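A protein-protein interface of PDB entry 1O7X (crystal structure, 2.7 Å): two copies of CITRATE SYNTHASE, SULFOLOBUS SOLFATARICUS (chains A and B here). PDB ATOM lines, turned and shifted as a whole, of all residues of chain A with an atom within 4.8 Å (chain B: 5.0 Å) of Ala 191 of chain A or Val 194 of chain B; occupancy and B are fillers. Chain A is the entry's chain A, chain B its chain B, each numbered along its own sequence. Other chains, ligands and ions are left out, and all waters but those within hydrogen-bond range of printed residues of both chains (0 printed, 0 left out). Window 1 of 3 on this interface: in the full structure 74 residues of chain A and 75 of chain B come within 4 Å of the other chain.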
ATOM      1  N   ALA A 187      12.844 -33.277 -21.873  1.00  0.00           N
ATOM      2  CA  ALA A 187      13.023 -32.082 -21.062  1.00  0.00           C
ATOM      3  C   ALA A 187      12.494 -32.259 -19.642  1.00  0.00           C
ATOM      4  O   ALA A 187      13.147 -31.784 -18.694  1.00  0.00           O
ATOM      5  CB  ALA A 187      12.413 -30.898 -21.766  1.00  0.00           C
ATOM      6  N   SER A 188      11.395 -32.991 -19.494  1.00  0.00           N
ATOM      7  CA  SER A 188      10.884 -33.238 -18.152  1.00  0.00           C
ATOM      8  C   SER A 188      11.823 -34.040 -17.266  1.00  0.00           C
ATOM      9  O   SER A 188      12.018 -33.676 -16.109  1.00  0.00           O
ATOM     10  CB  SER A 188       9.513 -33.903 -18.186  1.00  0.00           C
ATOM     11  OG  SER A 188       9.324 -35.116 -18.864  1.00  0.00           O
ATOM     12  N   THR A 189      12.436 -35.126 -17.710  1.00  0.00           N
ATOM     13  CA  THR A 189      13.305 -35.962 -16.896  1.00  0.00           C
ATOM     14  C   THR A 189      14.583 -35.182 -16.622  1.00  0.00           C
ATOM     15  O   THR A 189      15.154 -35.250 -15.537  1.00  0.00           O
ATOM     16  CB  THR A 189      13.638 -37.340 -17.531  1.00  0.00           C
ATOM     17  OG1 THR A 189      12.445 -37.971 -17.988  1.00  0.00           O
ATOM     18  CG2 THR A 189      14.268 -38.335 -16.560  1.00  0.00           C
ATOM     19  N   THR A 190      15.071 -34.508 -17.664  1.00  0.00           N
ATOM     20  CA  THR A 190      16.291 -33.719 -17.564  1.00  0.00           C
ATOM     21  C   THR A 190      16.100 -32.663 -16.476  1.00  0.00           C
ATOM     22  O   THR A 190      16.981 -32.584 -15.621  1.00  0.00           O
ATOM     23  CB  THR A 190      16.678 -32.997 -18.864  1.00  0.00           C
ATOM     24  OG1 THR A 190      16.911 -33.937 -19.917  1.00  0.00           O
ATOM     25  CG2 THR A 190      17.957 -32.210 -18.655  1.00  0.00           C
ATOM     26  N   ALA A 191      14.931 -31.990 -16.505  1.00  0.00           N
ATOM     27  CA  ALA A 191      14.717 -30.966 -15.489  1.00  0.00           C
ATOM     28  C   ALA A 191      14.592 -31.671 -14.153  1.00  0.00           C
ATOM     29  O   ALA A 191      15.276 -31.121 -13.277  1.00  0.00           O
ATOM     30  CB  ALA A 191      13.630 -29.933 -15.681  1.00  0.00           C
ATOM     31  N   ALA A 192      13.967 -32.817 -14.050  1.00  0.00           N
ATOM     32  CA  ALA A 192      14.026 -33.533 -12.773  1.00  0.00           C
ATOM     33  C   ALA A 192      15.454 -33.851 -12.358  1.00  0.00           C
ATOM     34  O   ALA A 192      15.751 -33.719 -11.164  1.00  0.00           O
ATOM     35  CB  ALA A 192      13.215 -34.821 -12.866  1.00  0.00           C
ATOM     36  N   LEU A 193      16.363 -34.231 -13.256  1.00  0.00           N
ATOM     37  CA  LEU A 193      17.719 -34.543 -12.853  1.00  0.00           C
ATOM     38  C   LEU A 193      18.495 -33.351 -12.330  1.00  0.00           C
ATOM     39  O   LEU A 193      19.235 -33.483 -11.341  1.00  0.00           O
ATOM     40  CB  LEU A 193      18.561 -35.172 -13.986  1.00  0.00           C
ATOM     41  CG  LEU A 193      17.893 -36.526 -14.338  1.00  0.00           C
ATOM     42  CD1 LEU A 193      17.954 -36.725 -15.829  1.00  0.00           C
ATOM     43  CD2 LEU A 193      18.505 -37.633 -13.496  1.00  0.00           C
ATOM     44  N   VAL A 194      18.330 -32.243 -13.075  1.00  0.00           N
ATOM     45  CA  VAL A 194      18.967 -30.992 -12.674  1.00  0.00           C
ATOM     46  C   VAL A 194      18.507 -30.630 -11.270  1.00  0.00           C
ATOM     47  O   VAL A 194      19.382 -30.348 -10.451  1.00  0.00           O
ATOM     48  CB  VAL A 194      18.682 -29.852 -13.662  1.00  0.00           C
ATOM     49  CG1 VAL A 194      19.226 -28.499 -13.177  1.00  0.00           C
ATOM     50  CG2 VAL A 194      19.198 -30.188 -15.064  1.00  0.00           C
ATOM     51  N   ALA A 195      17.227 -30.680 -10.947  1.00  0.00           N
ATOM     52  CA  ALA A 195      16.806 -30.318  -9.587  1.00  0.00           C
ATOM     53  C   ALA A 195      17.397 -31.252  -8.547  1.00  0.00           C
ATOM     54  O   ALA A 195      18.060 -30.847  -7.597  1.00  0.00           O
ATOM     55  CB  ALA A 195      15.300 -30.268  -9.425  1.00  0.00           C
ATOM     56  N   ALA A 208       9.814 -29.369 -11.178  1.00  0.00           N
ATOM     57  CA  ALA A 208      10.687 -29.045 -12.297  1.00  0.00           C
ATOM     58  C   ALA A 208      10.296 -29.783 -13.586  1.00  0.00           C
ATOM     59  O   ALA A 208      10.230 -29.145 -14.664  1.00  0.00           O
ATOM     60  CB  ALA A 208      12.130 -29.349 -11.928  1.00  0.00           C
ATOM     61  N   ALA A 209      10.084 -31.102 -13.533  1.00  0.00           N
ATOM     62  CA  ALA A 209       9.670 -31.917 -14.656  1.00  0.00           C
ATOM     63  C   ALA A 209       8.341 -31.450 -15.249  1.00  0.00           C
ATOM     64  O   ALA A 209       8.181 -31.341 -16.462  1.00  0.00           O
ATOM     65  CB  ALA A 209       9.420 -33.382 -14.306  1.00  0.00           C
ATOM     66  N   ALA A 212       8.599 -28.160 -17.245  1.00  0.00           N
ATOM     67  CA  ALA A 212       9.173 -28.341 -18.573  1.00  0.00           C
ATOM     68  C   ALA A 212       8.143 -29.043 -19.452  1.00  0.00           C
ATOM     69  O   ALA A 212       8.024 -28.643 -20.604  1.00  0.00           O
ATOM     70  CB  ALA A 212      10.481 -29.115 -18.609  1.00  0.00           C
ATOM     71  N   THR B 189      19.767 -21.825 -13.242  1.00  0.00           N
ATOM     72  CA  THR B 189      19.656 -21.345 -14.618  1.00  0.00           C
ATOM     73  C   THR B 189      19.471 -22.488 -15.608  1.00  0.00           C
ATOM     74  O   THR B 189      18.658 -22.369 -16.522  1.00  0.00           O
ATOM     75  CB  THR B 189      20.877 -20.477 -14.979  1.00  0.00           C
ATOM     76  OG1 THR B 189      20.950 -19.576 -13.860  1.00  0.00           O
ATOM     77  CG2 THR B 189      20.679 -19.745 -16.293  1.00  0.00           C
ATOM     78  N   THR B 190      20.177 -23.594 -15.378  1.00  0.00           N
ATOM     79  CA  THR B 190      20.083 -24.758 -16.247  1.00  0.00           C
ATOM     80  C   THR B 190      18.655 -25.271 -16.343  1.00  0.00           C
ATOM     81  O   THR B 190      18.056 -25.393 -17.416  1.00  0.00           O
ATOM     82  CB  THR B 190      21.049 -25.868 -15.785  1.00  0.00           C
ATOM     83  OG1 THR B 190      22.353 -25.243 -15.733  1.00  0.00           O
ATOM     84  CG2 THR B 190      21.094 -27.057 -16.735  1.00  0.00           C
ATOM     85  N   ALA B 191      18.054 -25.468 -15.180  1.00  0.00           N
ATOM     86  CA  ALA B 191      16.691 -25.960 -15.118  1.00  0.00           C
ATOM     87  C   ALA B 191      15.752 -24.938 -15.694  1.00  0.00           C
ATOM     88  O   ALA B 191      14.832 -25.359 -16.404  1.00  0.00           O
ATOM     89  CB  ALA B 191      16.425 -26.411 -13.703  1.00  0.00           C
ATOM     90  N   ALA B 192      16.001 -23.638 -15.591  1.00  0.00           N
ATOM     91  CA  ALA B 192      15.120 -22.658 -16.224  1.00  0.00           C
ATOM     92  C   ALA B 192      15.206 -22.786 -17.740  1.00  0.00           C
ATOM     93  O   ALA B 192      14.238 -22.715 -18.495  1.00  0.00           O
ATOM     94  CB  ALA B 192      15.505 -21.258 -15.780  1.00  0.00           C
ATOM     95  N   LEU B 193      16.436 -22.926 -18.226  1.00  0.00           N
ATOM     96  CA  LEU B 193      16.757 -23.119 -19.632  1.00  0.00           C
ATOM     97  C   LEU B 193      16.083 -24.385 -20.171  1.00  0.00           C
ATOM     98  O   LEU B 193      15.397 -24.436 -21.204  1.00  0.00           O
ATOM     99  CB  LEU B 193      18.274 -23.253 -19.789  1.00  0.00           C
ATOM    100  CG  LEU B 193      19.049 -21.928 -19.735  1.00  0.00           C
ATOM    101  CD1 LEU B 193      20.538 -22.223 -19.684  1.00  0.00           C
ATOM    102  CD2 LEU B 193      18.699 -21.023 -20.902  1.00  0.00           C
ATOM    103  N   VAL B 194      16.157 -25.430 -19.323  1.00  0.00           N
ATOM    104  CA  VAL B 194      15.488 -26.671 -19.717  1.00  0.00           C
ATOM    105  C   VAL B 194      14.006 -26.403 -19.812  1.00  0.00           C
ATOM    106  O   VAL B 194      13.442 -26.756 -20.853  1.00  0.00           O
ATOM    107  CB  VAL B 194      15.891 -27.869 -18.867  1.00  0.00           C
ATOM    108  CG1 VAL B 194      14.962 -29.053 -19.111  1.00  0.00           C
ATOM    109  CG2 VAL B 194      17.338 -28.203 -19.219  1.00  0.00           C
ATOM    110  N   ALA B 195      13.356 -25.768 -18.839  1.00  0.00           N
ATOM    111  CA  ALA B 195      11.907 -25.568 -19.015  1.00  0.00           C
ATOM    112  C   ALA B 195      11.600 -24.794 -20.287  1.00  0.00           C
ATOM    113  O   ALA B 195      10.778 -25.169 -21.112  1.00  0.00           O
ATOM    114  CB  ALA B 195      11.300 -24.910 -17.803  1.00  0.00           C
ATOM    115  N   ALA B 196      12.219 -23.635 -20.447  1.00  0.00           N
ATOM    116  CA  ALA B 196      12.098 -22.711 -21.555  1.00  0.00           C
ATOM    117  C   ALA B 196      12.373 -23.358 -22.907  1.00  0.00           C
ATOM    118  O   ALA B 196      11.738 -22.946 -23.899  1.00  0.00           O
ATOM    119  CB  ALA B 196      13.048 -21.550 -21.287  1.00  0.00           C
ATOM    120  N   SER B 197      13.242 -24.372 -23.046  1.00  0.00           N
ATOM    121  CA  SER B 197      13.436 -24.986 -24.348  1.00  0.00           C
ATOM    122  C   SER B 197      12.194 -25.748 -24.812  1.00  0.00           C
ATOM    123  O   SER B 197      12.104 -25.997 -26.028  1.00  0.00           O
ATOM    124  CB  SER B 197      14.658 -25.887 -24.367  1.00  0.00           C
ATOM    125  OG  SER B 197      14.394 -27.136 -23.712  1.00  0.00           O
ATOM    126  N   THR B 198      11.183 -26.058 -24.016  1.00  0.00           N
ATOM    127  CA  THR B 198       9.969 -26.717 -24.459  1.00  0.00           C
ATOM    128  C   THR B 198       8.866 -25.705 -24.777  1.00  0.00           C
ATOM    129  O   THR B 198       7.671 -26.007 -24.929  1.00  0.00           O
ATOM    130  CB  THR B 198       9.342 -27.656 -23.406  1.00  0.00           C
ATOM    131  OG1 THR B 198       8.877 -26.896 -22.272  1.00  0.00           O
ATOM    132  CG2 THR B 198      10.320 -28.705 -22.915  1.00  0.00           C
ATOM    133  N   ILE B 357      15.707 -29.262 -25.505  1.00  0.00           N
ATOM    134  CA  ILE B 357      16.809 -29.958 -24.858  1.00  0.00           C
ATOM    135  C   ILE B 357      16.481 -31.415 -24.618  1.00  0.00           C
ATOM    136  O   ILE B 357      15.630 -31.686 -23.777  1.00  0.00           O
ATOM    137  CB  ILE B 357      17.186 -29.227 -23.544  1.00  0.00           C
ATOM    138  CG1 ILE B 357      18.093 -28.030 -23.883  1.00  0.00           C
ATOM    139  CG2 ILE B 357      17.884 -30.127 -22.526  1.00  0.00           C
ATOM    140  CD1 ILE B 357      18.277 -27.004 -22.803  1.00  0.00           C
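O of Ala 212 of chain A lies within hydrogen-bond range of OG1 of Thr 198 of chain B (2.6 Å).
The backbone carbonyl oxygen of Val 194 of chain B sits at hydrogen-bond distance from the side-chain hydroxyl of Ser 197 of chain B, 3.0 Å away. The backbone carbonyl oxygen of Ala 195 of chain B lies within hydrogen-bond range of the side-chain hydroxyl of Thr 198 of chain B, 2.8 Å away. OG of Ser 197 of chain B is in hydrogen-bond range of N of Ile 357 of chain B, 3.1 Å away.
Among the printed residues, pairs that only touch across the chains: Ala 187 of chain A with Thr 198 of chain B (3.2 Å), Ala 187 of chain A with Val 194 of chain B (3.3 Å), Val 194 of chain A with Ala 191 of chain B (3.5 Å), Ala 187 of chain A with Ile 357 of chain B (3.7 Å), Ala 191 of chain A with Val 194 of chain B (3.8 Å) and Ala 212 of chain A with Ala 195 of chain B (3.8 Å).
Of the printed residues of chain B, Ala 187 of chain A touches Val 194 (3.3 Å), Thr 198 (3.2 Å) and Ile 357 (3.7 Å). Of the printed residues of chain B, Ala 191 of chain A touches Val 194. Of the printed residues of chain B, Val 194 of chain A touches Ala 191 (3.5 Å). Of the printed residues of chain A, Ala 191 of chain B touches Val 194. Of chain A, only Ala 187 and Ala 191 come within 4 Å of Val 194 of chain B. Of the printed residues of chain A, Ala 195 of chain B touches Ala 212 (3.8 Å). Printed residues of chain A within 4 Å of Thr 198 of chain B: Ala 187 and Ala 212. The nearest residue of chain A that does not touch Val 194 of chain B is Thr 190 of chain A (4.1 Å). The nearest printed residue of chain B that does not touch Val 194 of chain A is Thr 190 of chain B (4.02 Å).
Of the 11 printed residues of chain B, 5 touch a printed residue of chain A. Hydrophobic or aromatic side chains of chain B that line the printed part of chain A: Ala 191 and Val 194. Along chain B the printed residues that touch a printed residue of chain A span positions 191 to 357. Of the 12 printed residues of chain A, 4 touch a printed residue of chain B. Hydrophobic or aromatic side chains of chain A within 4 Å of the printed part of chain B: Ala 187, Ala 191, Val 194 and Ala 212.
Ala 191 of chain A touches Val 194 of chain B, and with the chains exchanged Val 194 of chain A touches Ala 191 of chain B. Of the 7 pairs that touch across the chains among the printed residues, 2 have their exchanged pair printed and touching as well.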
